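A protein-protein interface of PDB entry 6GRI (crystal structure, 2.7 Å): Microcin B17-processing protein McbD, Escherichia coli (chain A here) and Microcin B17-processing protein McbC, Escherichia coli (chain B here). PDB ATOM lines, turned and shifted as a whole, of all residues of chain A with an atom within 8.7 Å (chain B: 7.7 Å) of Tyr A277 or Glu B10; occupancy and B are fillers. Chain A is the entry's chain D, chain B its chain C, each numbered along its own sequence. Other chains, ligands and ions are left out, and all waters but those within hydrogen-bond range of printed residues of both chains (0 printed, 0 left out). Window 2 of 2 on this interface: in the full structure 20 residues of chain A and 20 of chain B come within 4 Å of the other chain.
OG of Ser B7 sits close to N of Val B9 (3.2 Å).
ND2 of Asn A3 sits at hydrogen-bond distance from OH of Tyr A5, 3.4 Å away.
The backbone carbonyl oxygen (O) of Gln A31 lies within hydrogen-bond range of the backbone NH (N) of Ala A17 (2.9 Å).
O of Phe A29 lies within hydrogen-bond range of N of Ser A19 (2.9 Å).
Of the 24 printed residues of chain A, 10 touch a printed residue of chain B.
Hydrophobic or aromatic side chains of chain A that line the printed part of chain B: Tyr A5, Ala A17, Pro A20, His A270, Ile A274 and Tyr A277.
Among the printed residues, no Asp or Glu carboxylate lies within 4 Å of a Lys or Arg side-chain nitrogen of the other chain.
Among the printed residues, pairs that only touch across the chains: Asn A3 with Thr B15 (3.5 Å), Tyr A5 with Thr B12 (3.9 Å), Tyr A5 with His B13 (3.5 Å), Tyr A5 with Tyr B14 (3.98 Å), Ala A17 with Thr B12 (3.8 Å), Ser A19 with Val B9 (3.0 Å), Pro A20 with Leu B8 (3.8 Å), Pro A20 with Thr B12 (3.8 Å), Gln A31 with Val B9 (3.9 Å), Asn A271 with Val B9 (3.98 Å) and Ile A274 with Glu B5 (3.6 Å).
Glu B10 touches one residue of chain A.
Of the printed residues of chain A, Ser B7 touches Asn A271.
Printed residues of chain A within 4 Å of Leu B8: Pro A20.
Of the printed residues of chain B, Asn A271 touches Ser B7 (3.3 Å) and Val B9 (3.98 Å).
Of the printed residues of chain B, His A270 touches Glu B5.
The nearest residue of chain B that does not touch Tyr A277 is Val B9 (7.3 Å).
NE2 of His A270 sits at hydrogen-bond distance from OE1 of Glu B5 (2.9 Å).
The side-chain hydroxyl of Ser B7 lies within hydrogen-bond range of the side-chain amide nitrogen of Asn A271 (3.3 Å).
The side-chain carboxylate (OE2) of Glu B10 is in hydrogen-bond range of the side-chain hydroxyl (OH) of Tyr A277 (2.8 Å).
O of Thr B12 is in hydrogen-bond range of ND2 of Asn A3 (2.8 Å).
OH of Tyr A5 is in hydrogen-bond range of O of Thr B15.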
ATOM      1  N   ASN A   3     -12.644 -11.549 -28.422  1.00  0.00           N
ATOM      2  CA  ASN A   3     -12.243 -12.932 -28.722  1.00  0.00           C
ATOM      3  C   ASN A   3     -11.061 -13.064 -29.688  1.00  0.00           C
ATOM      4  O   ASN A   3     -11.138 -13.776 -30.713  1.00  0.00           O
ATOM      5  CB  ASN A   3     -13.455 -13.728 -29.222  1.00  0.00           C
ATOM      6  CG  ASN A   3     -14.519 -13.897 -28.160  1.00  0.00           C
ATOM      7  OD1 ASN A   3     -15.664 -13.474 -28.337  1.00  0.00           O
ATOM      8  ND2 ASN A   3     -14.148 -14.525 -27.052  1.00  0.00           N
ATOM      9  N   TYR A   5      -7.454 -14.485 -30.406  1.00  0.00           N
ATOM     10  CA  TYR A   5      -6.664 -15.648 -30.068  1.00  0.00           C
ATOM     11  C   TYR A   5      -5.338 -15.531 -30.795  1.00  0.00           C
ATOM     12  O   TYR A   5      -5.284 -15.009 -31.911  1.00  0.00           O
ATOM     13  CB  TYR A   5      -7.393 -16.922 -30.489  1.00  0.00           C
ATOM     14  CG  TYR A   5      -8.818 -17.011 -29.977  1.00  0.00           C
ATOM     15  CD1 TYR A   5      -9.105 -16.927 -28.606  1.00  0.00           C
ATOM     16  CD2 TYR A   5      -9.888 -17.163 -30.861  1.00  0.00           C
ATOM     17  CE1 TYR A   5     -10.424 -17.003 -28.139  1.00  0.00           C
ATOM     18  CE2 TYR A   5     -11.202 -17.247 -30.411  1.00  0.00           C
ATOM     19  CZ  TYR A   5     -11.473 -17.174 -29.058  1.00  0.00           C
ATOM     20  OH  TYR A   5     -12.784 -17.261 -28.639  1.00  0.00           O
ATOM     21  N   ALA A  17     -10.646 -11.640 -24.016  1.00  0.00           N
ATOM     22  CA  ALA A  17     -12.094 -11.711 -24.156  1.00  0.00           C
ATOM     23  C   ALA A  17     -12.778 -10.694 -23.255  1.00  0.00           C
ATOM     24  O   ALA A  17     -12.389 -10.502 -22.113  1.00  0.00           O
ATOM     25  CB  ALA A  17     -12.589 -13.106 -23.830  1.00  0.00           C
ATOM     26  N   SER A  19     -16.254 -10.123 -21.425  1.00  0.00           N
ATOM     27  CA  SER A  19     -17.252 -11.061 -20.943  1.00  0.00           C
ATOM     28  C   SER A  19     -18.670 -10.641 -21.355  1.00  0.00           C
ATOM     29  O   SER A  19     -18.988  -9.452 -21.302  1.00  0.00           O
ATOM     30  CB  SER A  19     -17.180 -11.173 -19.435  1.00  0.00           C
ATOM     31  OG  SER A  19     -17.996 -12.241 -19.038  1.00  0.00           O
ATOM     32  N   PRO A  20     -19.532 -11.603 -21.758  1.00  0.00           N
ATOM     33  CA  PRO A  20     -20.921 -11.219 -22.004  1.00  0.00           C
ATOM     34  C   PRO A  20     -21.629 -11.104 -20.683  1.00  0.00           C
ATOM     35  O   PRO A  20     -21.165 -11.678 -19.714  1.00  0.00           O
ATOM     36  CB  PRO A  20     -21.499 -12.386 -22.836  1.00  0.00           C
ATOM     37  CG  PRO A  20     -20.429 -13.423 -22.925  1.00  0.00           C
ATOM     38  CD  PRO A  20     -19.338 -13.052 -21.949  1.00  0.00           C
ATOM     39  N   PHE A  29     -16.607  -6.804 -17.748  1.00  0.00           N
ATOM     40  CA  PHE A  29     -15.392  -7.431 -17.243  1.00  0.00           C
ATOM     41  C   PHE A  29     -14.610  -7.923 -18.467  1.00  0.00           C
ATOM     42  O   PHE A  29     -15.072  -8.791 -19.190  1.00  0.00           O
ATOM     43  CB  PHE A  29     -15.790  -8.592 -16.325  1.00  0.00           C
ATOM     44  CG  PHE A  29     -14.636  -9.363 -15.756  1.00  0.00           C
ATOM     45  CD1 PHE A  29     -14.052  -8.985 -14.550  1.00  0.00           C
ATOM     46  CD2 PHE A  29     -14.152 -10.504 -16.409  1.00  0.00           C
ATOM     47  CE1 PHE A  29     -12.987  -9.705 -14.023  1.00  0.00           C
ATOM     48  CE2 PHE A  29     -13.082 -11.228 -15.891  1.00  0.00           C
ATOM     49  CZ  PHE A  29     -12.498 -10.826 -14.694  1.00  0.00           C
ATOM     50  N   GLN A  31     -10.818  -9.492 -19.882  1.00  0.00           N
ATOM     51  CA  GLN A  31      -9.808 -10.382 -19.328  1.00  0.00           C
ATOM     52  C   GLN A  31      -8.849 -10.905 -20.394  1.00  0.00           C
ATOM     53  O   GLN A  31      -9.248 -11.160 -21.523  1.00  0.00           O
ATOM     54  CB  GLN A  31     -10.500 -11.552 -18.650  1.00  0.00           C
ATOM     55  CG  GLN A  31      -9.620 -12.356 -17.716  1.00  0.00           C
ATOM     56  CD  GLN A  31     -10.376 -13.516 -17.102  1.00  0.00           C
ATOM     57  OE1 GLN A  31     -10.877 -14.396 -17.821  1.00  0.00           O
ATOM     58  NE2 GLN A  31     -10.478 -13.521 -15.769  1.00  0.00           N
ATOM     59  N   TRP A  33      -5.690 -13.851 -20.906  1.00  0.00           N
ATOM     60  CA  TRP A  33      -5.240 -15.124 -20.362  1.00  0.00           C
ATOM     61  C   TRP A  33      -4.065 -15.648 -21.194  1.00  0.00           C
ATOM     62  O   TRP A  33      -4.156 -15.695 -22.428  1.00  0.00           O
ATOM     63  CB  TRP A  33      -6.401 -16.136 -20.361  1.00  0.00           C
ATOM     64  CG  TRP A  33      -6.062 -17.444 -19.666  1.00  0.00           C
ATOM     65  CD1 TRP A  33      -6.222 -17.731 -18.337  1.00  0.00           C
ATOM     66  CD2 TRP A  33      -5.494 -18.628 -20.266  1.00  0.00           C
ATOM     67  NE1 TRP A  33      -5.789 -19.016 -18.072  1.00  0.00           N
ATOM     68  CE2 TRP A  33      -5.338 -19.587 -19.233  1.00  0.00           C
ATOM     69  CE3 TRP A  33      -5.094 -18.968 -21.572  1.00  0.00           C
ATOM     70  CZ2 TRP A  33      -4.800 -20.864 -19.465  1.00  0.00           C
ATOM     71  CZ3 TRP A  33      -4.560 -20.240 -21.802  1.00  0.00           C
ATOM     72  CH2 TRP A  33      -4.419 -21.169 -20.752  1.00  0.00           C
ATOM     73  N   CYS A 268     -14.300 -12.506  -9.640  1.00  0.00           N
ATOM     74  CA  CYS A 268     -13.237 -13.432 -10.069  1.00  0.00           C
ATOM     75  C   CYS A 268     -13.101 -14.614  -9.159  1.00  0.00           C
ATOM     76  O   CYS A 268     -13.027 -15.741  -9.625  1.00  0.00           O
ATOM     77  CB  CYS A 268     -11.890 -12.755 -10.170  1.00  0.00           C
ATOM     78  SG  CYS A 268     -11.863 -11.611 -11.534  1.00  0.00           S
ATOM     79  N   LEU A 269     -13.077 -14.361  -7.863  1.00  0.00           N
ATOM     80  CA  LEU A 269     -12.993 -15.453  -6.910  1.00  0.00           C
ATOM     81  C   LEU A 269     -14.256 -16.319  -6.980  1.00  0.00           C
ATOM     82  O   LEU A 269     -14.154 -17.542  -7.044  1.00  0.00           O
ATOM     83  CB  LEU A 269     -12.743 -14.940  -5.491  1.00  0.00           C
ATOM     84  CG  LEU A 269     -12.482 -15.999  -4.411  1.00  0.00           C
ATOM     85  CD1 LEU A 269     -11.582 -17.144  -4.871  1.00  0.00           C
ATOM     86  CD2 LEU A 269     -11.884 -15.310  -3.192  1.00  0.00           C
ATOM     87  N   HIS A 270     -15.431 -15.685  -7.021  1.00  0.00           N
ATOM     88  CA  HIS A 270     -16.691 -16.421  -7.122  1.00  0.00           C
ATOM     89  C   HIS A 270     -16.614 -17.420  -8.267  1.00  0.00           C
ATOM     90  O   HIS A 270     -16.865 -18.605  -8.060  1.00  0.00           O
ATOM     91  CB  HIS A 270     -17.902 -15.503  -7.312  1.00  0.00           C
ATOM     92  CG  HIS A 270     -19.176 -16.252  -7.547  1.00  0.00           C
ATOM     93  ND1 HIS A 270     -19.855 -16.894  -6.536  1.00  0.00           N
ATOM     94  CD2 HIS A 270     -19.865 -16.505  -8.687  1.00  0.00           C
ATOM     95  CE1 HIS A 270     -20.915 -17.501  -7.044  1.00  0.00           C
ATOM     96  NE2 HIS A 270     -20.945 -17.279  -8.345  1.00  0.00           N
ATOM     97  N   ASN A 271     -16.233 -16.932  -9.451  1.00  0.00           N
ATOM     98  CA  ASN A 271     -16.052 -17.771 -10.644  1.00  0.00           C
ATOM     99  C   ASN A 271     -14.954 -18.821 -10.449  1.00  0.00           C
ATOM    100  O   ASN A 271     -15.155 -19.986 -10.765  1.00  0.00           O
ATOM    101  CB  ASN A 271     -15.746 -16.896 -11.870  1.00  0.00           C
ATOM    102  CG  ASN A 271     -16.967 -16.117 -12.369  1.00  0.00           C
ATOM    103  OD1 ASN A 271     -18.105 -16.374 -11.961  1.00  0.00           O
ATOM    104  ND2 ASN A 271     -16.731 -15.176 -13.274  1.00  0.00           N
ATOM    105  N   PHE A 272     -13.807 -18.422  -9.905  1.00  0.00           N
ATOM    106  CA  PHE A 272     -12.764 -19.388  -9.546  1.00  0.00           C
ATOM    107  C   PHE A 272     -13.371 -20.532  -8.737  1.00  0.00           C
ATOM    108  O   PHE A 272     -13.140 -21.700  -9.044  1.00  0.00           O
ATOM    109  CB  PHE A 272     -11.616 -18.736  -8.750  1.00  0.00           C
ATOM    110  CG  PHE A 272     -10.444 -19.655  -8.518  1.00  0.00           C
ATOM    111  CD1 PHE A 272     -10.377 -20.456  -7.377  1.00  0.00           C
ATOM    112  CD2 PHE A 272      -9.411 -19.740  -9.451  1.00  0.00           C
ATOM    113  CE1 PHE A 272      -9.303 -21.316  -7.175  1.00  0.00           C
ATOM    114  CE2 PHE A 272      -8.335 -20.597  -9.255  1.00  0.00           C
ATOM    115  CZ  PHE A 272      -8.283 -21.384  -8.117  1.00  0.00           C
ATOM    116  N   LEU A 273     -14.166 -20.178  -7.727  1.00  0.00           N
ATOM    117  CA  LEU A 273     -14.776 -21.157  -6.825  1.00  0.00           C
ATOM    118  C   LEU A 273     -15.791 -22.072  -7.512  1.00  0.00           C
ATOM    119  O   LEU A 273     -15.615 -23.283  -7.487  1.00  0.00           O
ATOM    120  CB  LEU A 273     -15.399 -20.463  -5.604  1.00  0.00           C
ATOM    121  CG  LEU A 273     -14.368 -19.820  -4.657  1.00  0.00           C
ATOM    122  CD1 LEU A 273     -15.020 -18.792  -3.751  1.00  0.00           C
ATOM    123  CD2 LEU A 273     -13.636 -20.860  -3.828  1.00  0.00           C
ATOM    124  N   ILE A 274     -16.825 -21.507  -8.136  1.00  0.00           N
ATOM    125  CA  ILE A 274     -17.860 -22.319  -8.824  1.00  0.00           C
ATOM    126  C   ILE A 274     -17.361 -23.131 -10.020  1.00  0.00           C
ATOM    127  O   ILE A 274     -17.981 -24.132 -10.364  1.00  0.00           O
ATOM    128  CB  ILE A 274     -19.107 -21.511  -9.284  1.00  0.00           C
ATOM    129  CG1 ILE A 274     -18.759 -20.449 -10.332  1.00  0.00           C
ATOM    130  CG2 ILE A 274     -19.813 -20.881  -8.092  1.00  0.00           C
ATOM    131  CD1 ILE A 274     -19.972 -19.778 -10.942  1.00  0.00           C
ATOM    132  N   GLY A 275     -16.263 -22.710 -10.644  1.00  0.00           N
ATOM    133  CA  GLY A 275     -15.684 -23.434 -11.778  1.00  0.00           C
ATOM    134  C   GLY A 275     -14.995 -24.768 -11.491  1.00  0.00           C
ATOM    135  O   GLY A 275     -14.683 -25.510 -12.427  1.00  0.00           O
ATOM    136  N   GLY A 276     -14.756 -25.081 -10.216  1.00  0.00           N
ATOM    137  CA  GLY A 276     -14.017 -26.286  -9.838  1.00  0.00           C
ATOM    138  C   GLY A 276     -12.507 -26.124  -9.927  1.00  0.00           C
ATOM    139  O   GLY A 276     -11.774 -27.113  -9.882  1.00  0.00           O
ATOM    140  N   TYR A 277     -12.033 -24.881 -10.027  1.00  0.00           N
ATOM    141  CA  TYR A 277     -10.598 -24.607 -10.091  1.00  0.00           C
ATOM    142  C   TYR A 277      -9.969 -24.964  -8.747  1.00  0.00           C
ATOM    143  O   TYR A 277     -10.540 -24.670  -7.696  1.00  0.00           O
ATOM    144  CB  TYR A 277     -10.319 -23.139 -10.457  1.00  0.00           C
ATOM    145  CG  TYR A 277     -10.745 -22.798 -11.865  1.00  0.00           C
ATOM    146  CD1 TYR A 277      -9.901 -23.042 -12.950  1.00  0.00           C
ATOM    147  CD2 TYR A 277     -11.999 -22.257 -12.122  1.00  0.00           C
ATOM    148  CE1 TYR A 277     -10.293 -22.747 -14.247  1.00  0.00           C
ATOM    149  CE2 TYR A 277     -12.402 -21.961 -13.414  1.00  0.00           C
ATOM    150  CZ  TYR A 277     -11.548 -22.205 -14.473  1.00  0.00           C
ATOM    151  OH  TYR A 277     -11.964 -21.908 -15.747  1.00  0.00           O
ATOM    152  N   THR A 278      -8.806 -25.613  -8.801  1.00  0.00           N
ATOM    153  CA  THR A 278      -8.117 -26.138  -7.617  1.00  0.00           C
ATOM    154  C   THR A 278      -6.960 -25.232  -7.156  1.00  0.00           C
ATOM    155  O   THR A 278      -6.616 -24.255  -7.827  1.00  0.00           O
ATOM    156  CB  THR A 278      -7.564 -27.540  -7.922  1.00  0.00           C
ATOM    157  OG1 THR A 278      -6.655 -27.458  -9.028  1.00  0.00           O
ATOM    158  CG2 THR A 278      -8.700 -28.490  -8.278  1.00  0.00           C
ATOM    159  N   ASP A 279      -6.359 -25.569  -6.015  1.00  0.00           N
ATOM    160  CA  ASP A 279      -5.181 -24.844  -5.495  1.00  0.00           C
ATOM    161  C   ASP A 279      -4.040 -24.741  -6.528  1.00  0.00           C
ATOM    162  O   ASP A 279      -3.355 -23.711  -6.593  1.00  0.00           O
ATOM    163  CB  ASP A 279      -4.662 -25.495  -4.202  1.00  0.00           C
ATOM    164  N   ASP A 280      -3.869 -25.798  -7.338  1.00  0.00           N
ATOM    165  CA  ASP A 280      -2.867 -25.844  -8.421  1.00  0.00           C
ATOM    166  C   ASP A 280      -3.046 -24.776  -9.518  1.00  0.00           C
ATOM    167  O   ASP A 280      -2.120 -24.542 -10.298  1.00  0.00           O
ATOM    168  CB  ASP A 280      -2.844 -27.235  -9.067  1.00  0.00           C
ATOM    169  N   ASP A 281      -4.229 -24.158  -9.586  1.00  0.00           N
ATOM    170  CA  ASP A 281      -4.481 -23.007 -10.459  1.00  0.00           C
ATOM    171  C   ASP A 281      -4.001 -21.694  -9.830  1.00  0.00           C
ATOM    172  O   ASP A 281      -3.460 -20.840 -10.526  1.00  0.00           O
ATOM    173  CB  ASP A 281      -5.972 -22.920 -10.817  1.00  0.00           C
ATOM    174  CG  ASP A 281      -6.471 -24.146 -11.596  1.00  0.00           C
ATOM    175  OD1 ASP A 281      -5.906 -24.445 -12.672  1.00  0.00           O
ATOM    176  OD2 ASP A 281      -7.431 -24.810 -11.143  1.00  0.00           O
ATOM    177  N   ILE A 282      -4.198 -21.535  -8.520  1.00  0.00           N
ATOM    178  CA  ILE A 282      -3.719 -20.351  -7.791  1.00  0.00           C
ATOM    179  C   ILE A 282      -2.188 -20.365  -7.664  1.00  0.00           C
ATOM    180  O   ILE A 282      -1.629 -21.192  -6.940  1.00  0.00           O
ATOM    181  CB  ILE A 282      -4.345 -20.262  -6.382  1.00  0.00           C
ATOM    182  N   MET A 291      -7.525 -15.713  -0.751  1.00  0.00           N
ATOM    183  CA  MET A 291      -8.470 -16.825  -0.715  1.00  0.00           C
ATOM    184  C   MET A 291      -8.622 -17.411   0.681  1.00  0.00           C
ATOM    185  O   MET A 291      -9.728 -17.764   1.083  1.00  0.00           O
ATOM    186  CB  MET A 291      -8.040 -17.930  -1.662  1.00  0.00           C
ATOM    187  CG  MET A 291      -8.195 -17.574  -3.120  1.00  0.00           C
ATOM    188  SD  MET A 291      -7.559 -18.893  -4.155  1.00  0.00           S
ATOM    189  CE  MET A 291      -8.621 -20.254  -3.659  1.00  0.00           C
ATOM    190  N   GLU B   5     -24.915 -22.691 -11.113  1.00  0.00           N
ATOM    191  CA  GLU B   5     -24.548 -21.472 -11.831  1.00  0.00           C
ATOM    192  C   GLU B   5     -23.492 -21.758 -12.887  1.00  0.00           C
ATOM    193  O   GLU B   5     -22.597 -22.569 -12.680  1.00  0.00           O
ATOM    194  CB  GLU B   5     -24.055 -20.382 -10.860  1.00  0.00           C
ATOM    195  CG  GLU B   5     -23.506 -19.120 -11.530  1.00  0.00           C
ATOM    196  CD  GLU B   5     -23.410 -17.904 -10.608  1.00  0.00           C
ATOM    197  OE1 GLU B   5     -23.565 -18.050  -9.375  1.00  0.00           O
ATOM    198  OE2 GLU B   5     -23.171 -16.787 -11.131  1.00  0.00           O
ATOM    199  N   LEU B   6     -23.635 -21.107 -14.036  1.00  0.00           N
ATOM    200  CA  LEU B   6     -22.634 -21.140 -15.096  1.00  0.00           C
ATOM    201  C   LEU B   6     -22.268 -19.701 -15.358  1.00  0.00           C
ATOM    202  O   LEU B   6     -23.164 -18.856 -15.538  1.00  0.00           O
ATOM    203  CB  LEU B   6     -23.211 -21.767 -16.365  1.00  0.00           C
ATOM    204  CG  LEU B   6     -22.378 -21.694 -17.641  1.00  0.00           C
ATOM    205  CD1 LEU B   6     -21.116 -22.523 -17.512  1.00  0.00           C
ATOM    206  CD2 LEU B   6     -23.192 -22.175 -18.820  1.00  0.00           C
ATOM    207  N   SER B   7     -20.967 -19.419 -15.367  1.00  0.00           N
ATOM    208  CA  SER B   7     -20.483 -18.106 -15.754  1.00  0.00           C
ATOM    209  C   SER B   7     -20.322 -18.046 -17.273  1.00  0.00           C
ATOM    210  O   SER B   7     -19.680 -18.902 -17.858  1.00  0.00           O
ATOM    211  CB  SER B   7     -19.152 -17.812 -15.089  1.00  0.00           C
ATOM    212  OG  SER B   7     -18.627 -16.594 -15.590  1.00  0.00           O
ATOM    213  N   LEU B   8     -20.888 -17.024 -17.907  1.00  0.00           N
ATOM    214  CA  LEU B   8     -20.660 -16.780 -19.339  1.00  0.00           C
ATOM    215  C   LEU B   8     -19.192 -16.533 -19.732  1.00  0.00           C
ATOM    216  O   LEU B   8     -18.835 -16.721 -20.888  1.00  0.00           O
ATOM    217  CB  LEU B   8     -21.510 -15.606 -19.828  1.00  0.00           C
ATOM    218  CG  LEU B   8     -23.026 -15.797 -19.823  1.00  0.00           C
ATOM    219  CD1 LEU B   8     -23.707 -14.478 -20.176  1.00  0.00           C
ATOM    220  CD2 LEU B   8     -23.446 -16.920 -20.778  1.00  0.00           C
ATOM    221  N   VAL B   9     -18.349 -16.125 -18.781  1.00  0.00           N
ATOM    222  CA  VAL B   9     -16.909 -15.960 -19.028  1.00  0.00           C
ATOM    223  C   VAL B   9     -16.292 -17.298 -19.467  1.00  0.00           C
ATOM    224  O   VAL B   9     -15.350 -17.319 -20.258  1.00  0.00           O
ATOM    225  CB  VAL B   9     -16.138 -15.494 -17.764  1.00  0.00           C
ATOM    226  CG1 VAL B   9     -14.670 -15.234 -18.091  1.00  0.00           C
ATOM    227  CG2 VAL B   9     -16.739 -14.239 -17.139  1.00  0.00           C
ATOM    228  N   GLU B  10     -16.799 -18.402 -18.907  1.00  0.00           N
ATOM    229  CA  GLU B  10     -16.415 -19.752 -19.326  1.00  0.00           C
ATOM    230  C   GLU B  10     -16.885 -20.017 -20.763  1.00  0.00           C
ATOM    231  O   GLU B  10     -16.139 -20.578 -21.563  1.00  0.00           O
ATOM    232  CB  GLU B  10     -17.016 -20.809 -18.403  1.00  0.00           C
ATOM    233  CG  GLU B  10     -16.576 -20.753 -16.954  1.00  0.00           C
ATOM    234  CD  GLU B  10     -15.165 -21.262 -16.715  1.00  0.00           C
ATOM    235  OE1 GLU B  10     -14.690 -22.150 -17.447  1.00  0.00           O
ATOM    236  OE2 GLU B  10     -14.523 -20.780 -15.761  1.00  0.00           O
ATOM    237  N   VAL B  11     -18.122 -19.623 -21.073  1.00  0.00           N
ATOM    238  CA  VAL B  11     -18.669 -19.756 -22.419  1.00  0.00           C
ATOM    239  C   VAL B  11     -17.798 -18.990 -23.416  1.00  0.00           C
ATOM    240  O   VAL B  11     -17.314 -19.574 -24.383  1.00  0.00           O
ATOM    241  CB  VAL B  11     -20.160 -19.306 -22.491  1.00  0.00           C
ATOM    242  CG1 VAL B  11     -20.634 -19.119 -23.932  1.00  0.00           C
ATOM    243  CG2 VAL B  11     -21.058 -20.310 -21.773  1.00  0.00           C
ATOM    244  N   THR B  12     -17.552 -17.711 -23.139  1.00  0.00           N
ATOM    245  CA  THR B  12     -16.855 -16.825 -24.076  1.00  0.00           C
ATOM    246  C   THR B  12     -15.432 -17.231 -24.458  1.00  0.00           C
ATOM    247  O   THR B  12     -14.890 -16.700 -25.410  1.00  0.00           O
ATOM    248  CB  THR B  12     -16.851 -15.360 -23.601  1.00  0.00           C
ATOM    249  OG1 THR B  12     -16.848 -14.494 -24.739  1.00  0.00           O
ATOM    250  CG2 THR B  12     -15.634 -15.029 -22.706  1.00  0.00           C
ATOM    251  N   HIS B  13     -14.835 -18.157 -23.722  1.00  0.00           N
ATOM    252  CA  HIS B  13     -13.544 -18.751 -24.081  1.00  0.00           C
ATOM    253  C   HIS B  13     -13.546 -19.530 -25.421  1.00  0.00           C
ATOM    254  O   HIS B  13     -12.503 -19.662 -26.042  1.00  0.00           O
ATOM    255  CB  HIS B  13     -13.096 -19.653 -22.916  1.00  0.00           C
ATOM    256  CG  HIS B  13     -11.747 -20.275 -23.088  1.00  0.00           C
ATOM    257  ND1 HIS B  13     -10.585 -19.655 -22.681  1.00  0.00           N
ATOM    258  CD2 HIS B  13     -11.377 -21.475 -23.599  1.00  0.00           C
ATOM    259  CE1 HIS B  13      -9.556 -20.441 -22.948  1.00  0.00           C
ATOM    260  NE2 HIS B  13     -10.008 -21.551 -23.508  1.00  0.00           N
ATOM    261  N   TYR B  14     -14.698 -20.047 -25.853  1.00  0.00           N
ATOM    262  CA  TYR B  14     -14.810 -20.855 -27.078  1.00  0.00           C
ATOM    263  C   TYR B  14     -15.522 -20.125 -28.220  1.00  0.00           C
ATOM    264  O   TYR B  14     -15.897 -20.745 -29.217  1.00  0.00           O
ATOM    265  CB  TYR B  14     -15.578 -22.149 -26.775  1.00  0.00           C
ATOM    266  CG  TYR B  14     -14.868 -23.062 -25.813  1.00  0.00           C
ATOM    267  CD1 TYR B  14     -13.989 -24.033 -26.281  1.00  0.00           C
ATOM    268  CD2 TYR B  14     -15.073 -22.965 -24.427  1.00  0.00           C
ATOM    269  CE1 TYR B  14     -13.331 -24.871 -25.407  1.00  0.00           C
ATOM    270  CE2 TYR B  14     -14.413 -23.806 -23.548  1.00  0.00           C
ATOM    271  CZ  TYR B  14     -13.541 -24.750 -24.045  1.00  0.00           C
ATOM    272  OH  TYR B  14     -12.871 -25.593 -23.205  1.00  0.00           O
ATOM    273  N   THR B  15     -15.710 -18.819 -28.089  1.00  0.00           N
ATOM    274  CA  THR B  15     -16.518 -18.078 -29.039  1.00  0.00           C
ATOM    275  C   THR B  15     -15.731 -17.716 -30.272  1.00  0.00           C
ATOM    276  O   THR B  15     -14.687 -17.079 -30.182  1.00  0.00           O
ATOM    277  CB  THR B  15     -17.045 -16.784 -28.414  1.00  0.00           C
ATOM    278  OG1 THR B  15     -17.895 -17.122 -27.318  1.00  0.00           O
ATOM    279  CG2 THR B  15     -17.824 -15.933 -29.448  1.00  0.00           C
ATOM    280  N   PHE B 200     -21.394 -21.234 -29.094  1.00  0.00           N
ATOM    281  CA  PHE B 200     -20.030 -21.668 -28.715  1.00  0.00           C
ATOM    282  C   PHE B 200     -19.653 -23.129 -28.979  1.00  0.00           C
ATOM    283  O   PHE B 200     -18.483 -23.416 -29.178  1.00  0.00           O
ATOM    284  CB  PHE B 200     -19.656 -21.252 -27.271  1.00  0.00           C
ATOM    285  CG  PHE B 200     -20.192 -22.158 -26.182  1.00  0.00           C
ATOM    286  CD1 PHE B 200     -21.558 -22.383 -26.034  1.00  0.00           C
ATOM    287  CD2 PHE B 200     -19.318 -22.737 -25.260  1.00  0.00           C
ATOM    288  CE1 PHE B 200     -22.028 -23.194 -25.014  1.00  0.00           C
ATOM    289  CE2 PHE B 200     -19.787 -23.548 -24.238  1.00  0.00           C
ATOM    290  CZ  PHE B 200     -21.141 -23.779 -24.112  1.00  0.00           C
